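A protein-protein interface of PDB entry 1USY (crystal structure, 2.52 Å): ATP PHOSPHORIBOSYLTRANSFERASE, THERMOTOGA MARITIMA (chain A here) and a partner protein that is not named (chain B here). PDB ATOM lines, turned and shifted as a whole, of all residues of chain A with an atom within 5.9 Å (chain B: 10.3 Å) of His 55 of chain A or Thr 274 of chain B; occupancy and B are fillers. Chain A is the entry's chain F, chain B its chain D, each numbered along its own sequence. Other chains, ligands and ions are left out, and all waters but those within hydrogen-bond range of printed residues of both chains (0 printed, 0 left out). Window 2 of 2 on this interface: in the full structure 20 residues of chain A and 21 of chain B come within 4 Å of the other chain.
The backbone NH (N) of Asp 243 of chain B lies within hydrogen-bond range of the backbone carbonyl oxygen (O) of Arg 248 of chain B, 2.7 Å away.
A ring nitrogen (ND1) of His 55 of chain A is in hydrogen-bond range of the backbone carbonyl oxygen (O) of Thr 51 of chain A, at 2.8 Å.
The backbone carbonyl oxygen of Leu 53 of chain A lies within hydrogen-bond range of the side-chain amide nitrogen of Asn 176 of chain A (2.9 Å).
The backbone NH (N) of Val 178 of chain A sits at hydrogen-bond distance from the side-chain amide oxygen (OD1) of Asn 176 of chain A (2.8 Å).
Of chain A, only Val 54, His 55, Asn 176 and Val 178 come within 4 Å of Thr 274 of chain B.
No residue of chain B comes within 4 Å of Thr 51 of chain A.
Val 54 of chain A touches just these residues of chain B: Thr 274 and Cys 275.
No residue of chain B comes within 4 Å of Gly 56 of chain A.
Printed residues of chain A within 4 Å of Cys 275 of chain B: Val 54 (3.7 Å), Pro 177 (3.4 Å) and Val 178 (3.6 Å).
Printed residues of chain B within 4 Å of Val 178 of chain A: Tyr 242 (3.8 Å), Ser 247 (3.4 Å), Arg 248 (3.8 Å), Thr 274 (3.7 Å) and Cys 275 (3.6 Å).
Of the printed residues of chain A, Ser 247 of chain B touches Val 178 (3.4 Å).
Of the printed residues of chain A, Arg 248 of chain B touches Val 178 (3.8 Å).
Of the printed residues of chain B, Asn 176 of chain A touches Thr 274.
Gly 272 of chain B touches none of the printed residues of chain A.
Among the printed residues, pairs that only touch across the chains: Pro 177 of chain A with Cys 275 of chain B (3.4 Å), Val 178 of chain A with Ser 247 of chain B (3.4 Å), Val 178 of chain A with Cys 275 of chain B (3.6 Å), His 55 of chain A with Thr 274 of chain B (3.6 Å), Val 54 of chain A with Cys 275 of chain B (3.7 Å), Val 178 of chain A with Thr 274 of chain B (3.7 Å), Val 178 of chain A with Arg 248 of chain B (3.8 Å) and Val 178 of chain A with Tyr 242 of chain B (3.8 Å).
The side-chain hydroxyl (OG1) of Thr 274 of chain B lies within hydrogen-bond range of the backbone carbonyl oxygen (O) of Val 54 of chain A, at 2.9 Å.
The side-chain amide nitrogen (ND2) of Asn 176 of chain A is in hydrogen-bond range of the backbone carbonyl oxygen (O) of Thr 274 of chain B (2.8 Å).
Of the 22 printed residues of chain B, 5 touch a printed residue of chain A.
Among the printed residues, 10 pairs touch across the chains.
Among the printed residues, no Asp or Glu carboxylate lies within 4 Å of a Lys or Arg side-chain nitrogen of the other chain.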
ATOM      1  N   PRO A  50     -18.309 -23.656   1.964  1.00  0.00           N
ATOM      2  CA  PRO A  50     -18.542 -22.947   0.704  1.00  0.00           C
ATOM      3  C   PRO A  50     -17.304 -22.286   0.124  1.00  0.00           C
ATOM      4  O   PRO A  50     -17.106 -22.372  -1.124  1.00  0.00           O
ATOM      5  CB  PRO A  50     -19.589 -21.890   1.072  1.00  0.00           C
ATOM      6  CG  PRO A  50     -20.244 -22.411   2.319  1.00  0.00           C
ATOM      7  CD  PRO A  50     -19.302 -23.303   2.990  1.00  0.00           C
ATOM      8  N   THR A  51     -16.498 -21.650   0.983  1.00  0.00           N
ATOM      9  CA  THR A  51     -15.292 -20.951   0.529  1.00  0.00           C
ATOM     10  C   THR A  51     -14.399 -21.890  -0.236  1.00  0.00           C
ATOM     11  O   THR A  51     -13.806 -21.512  -1.255  1.00  0.00           O
ATOM     12  CB  THR A  51     -14.481 -20.384   1.710  1.00  0.00           C
ATOM     13  OG1 THR A  51     -15.363 -19.704   2.615  1.00  0.00           O
ATOM     14  CG2 THR A  51     -13.571 -19.301   1.224  1.00  0.00           C
ATOM     15  N   TYR A  52     -14.301 -23.110   0.273  1.00  0.00           N
ATOM     16  CA  TYR A  52     -13.400 -24.099  -0.299  1.00  0.00           C
ATOM     17  C   TYR A  52     -13.927 -24.585  -1.649  1.00  0.00           C
ATOM     18  O   TYR A  52     -13.183 -24.717  -2.609  1.00  0.00           O
ATOM     19  CB  TYR A  52     -13.147 -25.242   0.676  1.00  0.00           C
ATOM     20  CG  TYR A  52     -12.068 -24.976   1.719  1.00  0.00           C
ATOM     21  CD1 TYR A  52     -12.273 -24.066   2.758  1.00  0.00           C
ATOM     22  CD2 TYR A  52     -10.876 -25.677   1.702  1.00  0.00           C
ATOM     23  CE1 TYR A  52     -11.328 -23.833   3.708  1.00  0.00           C
ATOM     24  CE2 TYR A  52      -9.908 -25.458   2.650  1.00  0.00           C
ATOM     25  CZ  TYR A  52     -10.129 -24.546   3.656  1.00  0.00           C
ATOM     26  OH  TYR A  52      -9.132 -24.353   4.601  1.00  0.00           O
ATOM     27  N   LEU A  53     -15.226 -24.775  -1.740  1.00  0.00           N
ATOM     28  CA  LEU A  53     -15.848 -25.164  -3.002  1.00  0.00           C
ATOM     29  C   LEU A  53     -15.790 -24.113  -4.072  1.00  0.00           C
ATOM     30  O   LEU A  53     -15.420 -24.433  -5.200  1.00  0.00           O
ATOM     31  CB  LEU A  53     -17.283 -25.576  -2.768  1.00  0.00           C
ATOM     32  CG  LEU A  53     -17.405 -26.840  -1.914  1.00  0.00           C
ATOM     33  CD1 LEU A  53     -18.834 -27.046  -1.538  1.00  0.00           C
ATOM     34  CD2 LEU A  53     -16.849 -28.058  -2.669  1.00  0.00           C
ATOM     35  N   VAL A  54     -16.152 -22.865  -3.755  1.00  0.00           N
ATOM     36  CA  VAL A  54     -16.227 -21.845  -4.819  1.00  0.00           C
ATOM     37  C   VAL A  54     -14.874 -21.415  -5.392  1.00  0.00           C
ATOM     38  O   VAL A  54     -14.813 -20.922  -6.533  1.00  0.00           O
ATOM     39  CB  VAL A  54     -17.033 -20.556  -4.460  1.00  0.00           C
ATOM     40  CG1 VAL A  54     -18.348 -20.840  -3.686  1.00  0.00           C
ATOM     41  CG2 VAL A  54     -16.165 -19.589  -3.744  1.00  0.00           C
ATOM     42  N   HIS A  55     -13.791 -21.573  -4.626  1.00  0.00           N
ATOM     43  CA  HIS A  55     -12.451 -21.289  -5.166  1.00  0.00           C
ATOM     44  C   HIS A  55     -11.900 -22.539  -5.858  1.00  0.00           C
ATOM     45  O   HIS A  55     -10.785 -22.520  -6.392  1.00  0.00           O
ATOM     46  CB  HIS A  55     -11.470 -20.863  -4.074  1.00  0.00           C
ATOM     47  CG  HIS A  55     -11.716 -19.505  -3.497  1.00  0.00           C
ATOM     48  ND1 HIS A  55     -12.630 -19.274  -2.487  1.00  0.00           N
ATOM     49  CD2 HIS A  55     -11.104 -18.318  -3.723  1.00  0.00           C
ATOM     50  CE1 HIS A  55     -12.590 -17.999  -2.135  1.00  0.00           C
ATOM     51  NE2 HIS A  55     -11.663 -17.401  -2.861  1.00  0.00           N
ATOM     52  N   GLY A  56     -12.680 -23.615  -5.845  1.00  0.00           N
ATOM     53  CA  GLY A  56     -12.304 -24.873  -6.475  1.00  0.00           C
ATOM     54  C   GLY A  56     -11.184 -25.640  -5.775  1.00  0.00           C
ATOM     55  O   GLY A  56     -10.612 -26.582  -6.347  1.00  0.00           O
ATOM     56  N   VAL A  57     -10.873 -25.227  -4.537  1.00  0.00           N
ATOM     57  CA  VAL A  57      -9.815 -25.857  -3.746  1.00  0.00           C
ATOM     58  C   VAL A  57     -10.302 -27.181  -3.172  1.00  0.00           C
ATOM     59  O   VAL A  57      -9.490 -28.055  -2.843  1.00  0.00           O
ATOM     60  CB  VAL A  57      -9.211 -24.923  -2.667  1.00  0.00           C
ATOM     61  CG1 VAL A  57      -8.580 -23.718  -3.325  1.00  0.00           C
ATOM     62  CG2 VAL A  57     -10.241 -24.486  -1.669  1.00  0.00           C
ATOM     63  N   ALA A  58     -11.618 -27.325  -3.080  1.00  0.00           N
ATOM     64  CA  ALA A  58     -12.242 -28.640  -2.935  1.00  0.00           C
ATOM     65  C   ALA A  58     -13.254 -28.873  -4.047  1.00  0.00           C
ATOM     66  O   ALA A  58     -13.753 -27.927  -4.664  1.00  0.00           O
ATOM     67  CB  ALA A  58     -12.889 -28.781  -1.595  1.00  0.00           C
ATOM     68  N   ASN A 176     -18.786 -28.553  -6.444  1.00  0.00           N
ATOM     69  CA  ASN A 176     -18.391 -27.409  -7.234  1.00  0.00           C
ATOM     70  C   ASN A 176     -18.819 -27.752  -8.671  1.00  0.00           C
ATOM     71  O   ASN A 176     -18.535 -28.864  -9.144  1.00  0.00           O
ATOM     72  CB  ASN A 176     -16.889 -27.216  -7.049  1.00  0.00           C
ATOM     73  CG  ASN A 176     -16.213 -26.528  -8.207  1.00  0.00           C
ATOM     74  OD1 ASN A 176     -16.274 -26.962  -9.369  1.00  0.00           O
ATOM     75  ND2 ASN A 176     -15.540 -25.452  -7.893  1.00  0.00           N
ATOM     76  N   PRO A 177     -19.537 -26.850  -9.344  1.00  0.00           N
ATOM     77  CA  PRO A 177     -20.133 -27.194 -10.635  1.00  0.00           C
ATOM     78  C   PRO A 177     -19.131 -27.386 -11.756  1.00  0.00           C
ATOM     79  O   PRO A 177     -19.491 -28.016 -12.743  1.00  0.00           O
ATOM     80  CB  PRO A 177     -21.064 -26.019 -10.957  1.00  0.00           C
ATOM     81  CG  PRO A 177     -20.953 -25.055  -9.855  1.00  0.00           C
ATOM     82  CD  PRO A 177     -19.829 -25.472  -8.930  1.00  0.00           C
ATOM     83  N   VAL A 178     -17.924 -26.853 -11.667  1.00  0.00           N
ATOM     84  CA  VAL A 178     -17.012 -27.138 -12.764  1.00  0.00           C
ATOM     85  C   VAL A 178     -16.417 -28.531 -12.603  1.00  0.00           C
ATOM     86  O   VAL A 178     -16.277 -29.258 -13.582  1.00  0.00           O
ATOM     87  CB  VAL A 178     -15.982 -25.988 -13.147  1.00  0.00           C
ATOM     88  CG1 VAL A 178     -16.526 -24.557 -12.785  1.00  0.00           C
ATOM     89  CG2 VAL A 178     -14.544 -26.272 -12.660  1.00  0.00           C
ATOM     90  N   ARG B  81     -15.820  -7.133 -11.428  1.00  0.00           N
ATOM     91  CA  ARG B  81     -16.878  -7.788 -10.651  1.00  0.00           C
ATOM     92  C   ARG B  81     -16.526  -7.782  -9.185  1.00  0.00           C
ATOM     93  O   ARG B  81     -15.370  -7.549  -8.808  1.00  0.00           O
ATOM     94  CB  ARG B  81     -17.196  -9.205 -11.185  1.00  0.00           C
ATOM     95  CG  ARG B  81     -16.786 -10.402 -10.289  1.00  0.00           C
ATOM     96  CD  ARG B  81     -15.736 -11.322 -10.887  1.00  0.00           C
ATOM     97  NE  ARG B  81     -16.158 -12.719 -11.058  1.00  0.00           N
ATOM     98  CZ  ARG B  81     -15.303 -13.762 -11.163  1.00  0.00           C
ATOM     99  NH1 ARG B  81     -13.980 -13.547 -11.107  1.00  0.00           N
ATOM    100  NH2 ARG B  81     -15.759 -15.020 -11.317  1.00  0.00           N
ATOM    101  N   SER B  83     -16.456  -9.746  -5.464  1.00  0.00           N
ATOM    102  CA  SER B  83     -16.588 -10.956  -4.668  1.00  0.00           C
ATOM    103  C   SER B  83     -16.539 -10.470  -3.231  1.00  0.00           C
ATOM    104  O   SER B  83     -15.500  -9.977  -2.769  1.00  0.00           O
ATOM    105  CB  SER B  83     -15.463 -11.957  -4.978  1.00  0.00           C
ATOM    106  OG  SER B  83     -14.190 -11.395  -4.686  1.00  0.00           O
ATOM    107  N   GLY B  84     -17.671 -10.565  -2.537  1.00  0.00           N
ATOM    108  CA  GLY B  84     -17.817  -9.830  -1.296  1.00  0.00           C
ATOM    109  C   GLY B  84     -17.670  -8.380  -1.695  1.00  0.00           C
ATOM    110  O   GLY B  84     -18.321  -7.925  -2.643  1.00  0.00           O
ATOM    111  N   ASP B  86     -14.841  -6.821  -2.837  1.00  0.00           N
ATOM    112  CA  ASP B  86     -13.546  -6.646  -3.473  1.00  0.00           C
ATOM    113  C   ASP B  86     -13.792  -6.438  -4.929  1.00  0.00           C
ATOM    114  O   ASP B  86     -14.571  -7.172  -5.531  1.00  0.00           O
ATOM    115  CB  ASP B  86     -12.678  -7.894  -3.289  1.00  0.00           C
ATOM    116  CG  ASP B  86     -11.841  -7.847  -2.025  1.00  0.00           C
ATOM    117  OD1 ASP B  86     -11.057  -6.876  -1.843  1.00  0.00           O
ATOM    118  OD2 ASP B  86     -11.901  -8.759  -1.165  1.00  0.00           O
ATOM    119  N   VAL B  88     -12.817  -6.995  -8.533  1.00  0.00           N
ATOM    120  CA  VAL B  88     -11.992  -8.009  -9.191  1.00  0.00           C
ATOM    121  C   VAL B  88     -12.120  -7.914 -10.708  1.00  0.00           C
ATOM    122  O   VAL B  88     -13.230  -7.763 -11.218  1.00  0.00           O
ATOM    123  CB  VAL B  88     -12.405  -9.481  -8.724  1.00  0.00           C
ATOM    124  CG1 VAL B  88     -12.072 -10.504  -9.786  1.00  0.00           C
ATOM    125  CG2 VAL B  88     -11.743  -9.867  -7.389  1.00  0.00           C
ATOM    126  N   GLU B  90     -11.070  -9.607 -14.711  1.00  0.00           N
ATOM    127  CA  GLU B  90     -10.637 -10.754 -15.505  1.00  0.00           C
ATOM    128  C   GLU B  90     -10.760 -10.456 -16.986  1.00  0.00           C
ATOM    129  O   GLU B  90     -11.783  -9.953 -17.475  1.00  0.00           O
ATOM    130  CB  GLU B  90     -11.454 -11.981 -15.170  1.00  0.00           C
ATOM    131  CG  GLU B  90     -12.899 -11.693 -14.854  1.00  0.00           C
ATOM    132  CD  GLU B  90     -13.814 -12.615 -15.628  1.00  0.00           C
ATOM    133  OE1 GLU B  90     -14.371 -12.169 -16.679  1.00  0.00           O
ATOM    134  OE2 GLU B  90     -13.952 -13.790 -15.183  1.00  0.00           O
ATOM    135  N   ILE B 241     -18.267 -23.634 -21.854  1.00  0.00           N
ATOM    136  CA  ILE B 241     -17.088 -24.461 -22.133  1.00  0.00           C
ATOM    137  C   ILE B 241     -16.264 -24.594 -20.875  1.00  0.00           C
ATOM    138  O   ILE B 241     -16.069 -23.613 -20.159  1.00  0.00           O
ATOM    139  CB  ILE B 241     -16.240 -23.876 -23.301  1.00  0.00           C
ATOM    140  CG1 ILE B 241     -17.148 -23.506 -24.477  1.00  0.00           C
ATOM    141  CG2 ILE B 241     -15.135 -24.821 -23.656  1.00  0.00           C
ATOM    142  CD1 ILE B 241     -16.433 -22.922 -25.678  1.00  0.00           C
ATOM    143  N   TYR B 242     -15.791 -25.807 -20.606  1.00  0.00           N
ATOM    144  CA  TYR B 242     -14.915 -26.071 -19.471  1.00  0.00           C
ATOM    145  C   TYR B 242     -13.604 -26.626 -19.983  1.00  0.00           C
ATOM    146  O   TYR B 242     -13.568 -27.323 -21.011  1.00  0.00           O
ATOM    147  CB  TYR B 242     -15.539 -27.096 -18.553  1.00  0.00           C
ATOM    148  CG  TYR B 242     -16.890 -26.726 -18.054  1.00  0.00           C
ATOM    149  CD1 TYR B 242     -18.025 -26.965 -18.829  1.00  0.00           C
ATOM    150  CD2 TYR B 242     -17.052 -26.161 -16.782  1.00  0.00           C
ATOM    151  CE1 TYR B 242     -19.292 -26.640 -18.365  1.00  0.00           C
ATOM    152  CE2 TYR B 242     -18.322 -25.815 -16.305  1.00  0.00           C
ATOM    153  CZ  TYR B 242     -19.423 -26.061 -17.103  1.00  0.00           C
ATOM    154  OH  TYR B 242     -20.661 -25.745 -16.637  1.00  0.00           O
ATOM    155  N   ASP B 243     -12.530 -26.317 -19.265  1.00  0.00           N
ATOM    156  CA  ASP B 243     -11.231 -26.886 -19.547  1.00  0.00           C
ATOM    157  C   ASP B 243     -10.931 -27.929 -18.462  1.00  0.00           C
ATOM    158  O   ASP B 243     -10.822 -27.571 -17.281  1.00  0.00           O
ATOM    159  CB  ASP B 243     -10.173 -25.783 -19.546  1.00  0.00           C
ATOM    160  CG  ASP B 243      -8.778 -26.311 -19.851  1.00  0.00           C
ATOM    161  OD1 ASP B 243      -8.683 -27.307 -20.615  1.00  0.00           O
ATOM    162  OD2 ASP B 243      -7.733 -25.817 -19.367  1.00  0.00           O
ATOM    163  N   SER B 246      -7.044 -27.639 -16.662  1.00  0.00           N
ATOM    164  CA  SER B 246      -6.988 -26.696 -15.563  1.00  0.00           C
ATOM    165  C   SER B 246      -8.228 -26.722 -14.648  1.00  0.00           C
ATOM    166  O   SER B 246      -8.283 -25.963 -13.695  1.00  0.00           O
ATOM    167  CB  SER B 246      -6.745 -25.282 -16.106  1.00  0.00           C
ATOM    168  OG  SER B 246      -7.835 -24.841 -16.916  1.00  0.00           O
ATOM    169  N   SER B 247      -9.189 -27.621 -14.922  1.00  0.00           N
ATOM    170  CA  SER B 247     -10.500 -27.712 -14.235  1.00  0.00           C
ATOM    171  C   SER B 247     -11.070 -26.352 -13.991  1.00  0.00           C
ATOM    172  O   SER B 247     -11.208 -25.908 -12.851  1.00  0.00           O
ATOM    173  CB  SER B 247     -10.395 -28.430 -12.901  1.00  0.00           C
ATOM    174  OG  SER B 247     -11.683 -28.766 -12.408  1.00  0.00           O
ATOM    175  N   ARG B 248     -11.355 -25.648 -15.063  1.00  0.00           N
ATOM    176  CA  ARG B 248     -12.104 -24.438 -14.885  1.00  0.00           C
ATOM    177  C   ARG B 248     -13.005 -24.071 -16.029  1.00  0.00           C
ATOM    178  O   ARG B 248     -12.916 -24.665 -17.123  1.00  0.00           O
ATOM    179  CB  ARG B 248     -11.225 -23.299 -14.393  1.00  0.00           C
ATOM    180  CG  ARG B 248      -9.990 -23.048 -15.091  1.00  0.00           C
ATOM    181  CD  ARG B 248      -9.418 -21.684 -14.675  1.00  0.00           C
ATOM    182  NE  ARG B 248      -8.774 -21.690 -13.349  1.00  0.00           N
ATOM    183  CZ  ARG B 248      -8.525 -20.597 -12.593  1.00  0.00           C
ATOM    184  NH1 ARG B 248      -7.921 -20.727 -11.415  1.00  0.00           N
ATOM    185  NH2 ARG B 248      -8.873 -19.377 -13.000  1.00  0.00           N
ATOM    186  N   LEU B 249     -13.932 -23.163 -15.724  1.00  0.00           N
ATOM    187  CA  LEU B 249     -14.948 -22.691 -16.660  1.00  0.00           C
ATOM    188  C   LEU B 249     -14.266 -21.692 -17.573  1.00  0.00           C
ATOM    189  O   LEU B 249     -13.739 -20.674 -17.128  1.00  0.00           O
ATOM    190  CB  LEU B 249     -16.116 -22.037 -15.915  1.00  0.00           C
ATOM    191  CG  LEU B 249     -17.153 -21.272 -16.741  1.00  0.00           C
ATOM    192  CD1 LEU B 249     -17.785 -22.216 -17.687  1.00  0.00           C
ATOM    193  CD2 LEU B 249     -18.207 -20.753 -15.820  1.00  0.00           C
ATOM    194  N   VAL B 250     -14.304 -21.977 -18.859  1.00  0.00           N
ATOM    195  CA  VAL B 250     -13.479 -21.259 -19.803  1.00  0.00           C
ATOM    196  C   VAL B 250     -14.243 -20.322 -20.766  1.00  0.00           C
ATOM    197  O   VAL B 250     -13.673 -19.409 -21.369  1.00  0.00           O
ATOM    198  CB  VAL B 250     -12.601 -22.318 -20.449  1.00  0.00           C
ATOM    199  CG1 VAL B 250     -12.693 -22.349 -21.948  1.00  0.00           C
ATOM    200  CG2 VAL B 250     -11.214 -22.187 -19.898  1.00  0.00           C
ATOM    201  N   ALA B 251     -15.550 -20.517 -20.897  1.00  0.00           N
ATOM    202  CA  ALA B 251     -16.323 -19.720 -21.832  1.00  0.00           C
ATOM    203  C   ALA B 251     -17.791 -19.896 -21.541  1.00  0.00           C
ATOM    204  O   ALA B 251     -18.168 -20.896 -20.975  1.00  0.00           O
ATOM    205  CB  ALA B 251     -16.046 -20.157 -23.228  1.00  0.00           C
ATOM    206  N   PHE B 269     -12.923 -16.528 -21.045  1.00  0.00           N
ATOM    207  CA  PHE B 269     -12.164 -15.999 -19.921  1.00  0.00           C
ATOM    208  C   PHE B 269     -10.792 -16.671 -19.907  1.00  0.00           C
ATOM    209  O   PHE B 269     -10.701 -17.860 -19.602  1.00  0.00           O
ATOM    210  CB  PHE B 269     -12.879 -16.291 -18.583  1.00  0.00           C
ATOM    211  CG  PHE B 269     -14.401 -16.316 -18.701  1.00  0.00           C
ATOM    212  CD1 PHE B 269     -15.106 -15.129 -18.912  1.00  0.00           C
ATOM    213  CD2 PHE B 269     -15.091 -17.524 -18.599  1.00  0.00           C
ATOM    214  CE1 PHE B 269     -16.503 -15.153 -19.027  1.00  0.00           C
ATOM    215  CE2 PHE B 269     -16.484 -17.550 -18.717  1.00  0.00           C
ATOM    216  CZ  PHE B 269     -17.190 -16.364 -18.932  1.00  0.00           C
ATOM    217  N   LEU B 270      -9.729 -15.889 -20.263  1.00  0.00           N
ATOM    218  CA  LEU B 270      -8.315 -16.416 -20.222  1.00  0.00           C
ATOM    219  C   LEU B 270      -7.979 -16.781 -18.767  1.00  0.00           C
ATOM    220  O   LEU B 270      -7.535 -15.919 -17.992  1.00  0.00           O
ATOM    221  CB  LEU B 270      -7.225 -15.394 -20.578  1.00  0.00           C
ATOM    222  CG  LEU B 270      -7.211 -14.699 -21.930  1.00  0.00           C
ATOM    223  CD1 LEU B 270      -6.144 -13.602 -21.912  1.00  0.00           C
ATOM    224  CD2 LEU B 270      -6.870 -15.611 -23.121  1.00  0.00           C
ATOM    225  N   GLU B 271      -8.173 -18.022 -18.419  1.00  0.00           N
ATOM    226  CA  GLU B 271      -8.002 -18.488 -17.027  1.00  0.00           C
ATOM    227  C   GLU B 271      -9.379 -18.353 -16.381  1.00  0.00           C
ATOM    228  O   GLU B 271     -10.349 -18.908 -16.879  1.00  0.00           O
ATOM    229  CB  GLU B 271      -6.991 -17.636 -16.293  1.00  0.00           C
ATOM    230  N   GLY B 272      -9.416 -17.611 -15.295  1.00  0.00           N
ATOM    231  CA  GLY B 272     -10.666 -17.279 -14.540  1.00  0.00           C
ATOM    232  C   GLY B 272     -11.712 -18.417 -14.488  1.00  0.00           C
ATOM    233  O   GLY B 272     -11.834 -19.256 -15.384  1.00  0.00           O
ATOM    234  N   LYS B 273     -12.531 -18.240 -13.452  1.00  0.00           N
ATOM    235  CA  LYS B 273     -13.715 -19.076 -13.218  1.00  0.00           C
ATOM    236  C   LYS B 273     -13.420 -20.511 -12.744  1.00  0.00           C
ATOM    237  O   LYS B 273     -13.133 -21.414 -13.507  1.00  0.00           O
ATOM    238  CB  LYS B 273     -14.682 -19.000 -14.400  1.00  0.00           C
ATOM    239  CG  LYS B 273     -14.984 -17.542 -14.808  1.00  0.00           C
ATOM    240  CD  LYS B 273     -16.346 -17.136 -14.387  1.00  0.00           C
ATOM    241  CE  LYS B 273     -16.799 -15.947 -15.196  1.00  0.00           C
ATOM    242  NZ  LYS B 273     -16.435 -14.709 -14.439  1.00  0.00           N
ATOM    243  N   THR B 274     -13.499 -20.656 -11.428  1.00  0.00           N
ATOM    244  CA  THR B 274     -13.372 -21.915 -10.739  1.00  0.00           C
ATOM    245  C   THR B 274     -14.777 -22.341 -10.324  1.00  0.00           C
ATOM    246  O   THR B 274     -14.947 -23.308  -9.583  1.00  0.00           O
ATOM    247  CB  THR B 274     -12.452 -21.713  -9.489  1.00  0.00           C
ATOM    248  OG1 THR B 274     -12.922 -20.606  -8.707  1.00  0.00           O
ATOM    249  CG2 THR B 274     -11.041 -21.254  -9.901  1.00  0.00           C
ATOM    250  N   CYS B 275     -15.784 -21.628 -10.828  1.00  0.00           N
ATOM    251  CA  CYS B 275     -17.129 -21.711 -10.273  1.00  0.00           C
ATOM    252  C   CYS B 275     -18.281 -21.645 -11.277  1.00  0.00           C
ATOM    253  O   CYS B 275     -18.398 -20.701 -12.085  1.00  0.00           O
ATOM    254  CB  CYS B 275     -17.314 -20.622  -9.211  1.00  0.00           C
ATOM    255  SG  CYS B 275     -18.412 -21.174  -7.907  1.00  0.00           S
ATOM    256  OXT CYS B 275     -19.083 -22.608 -11.185  1.00  0.00           O
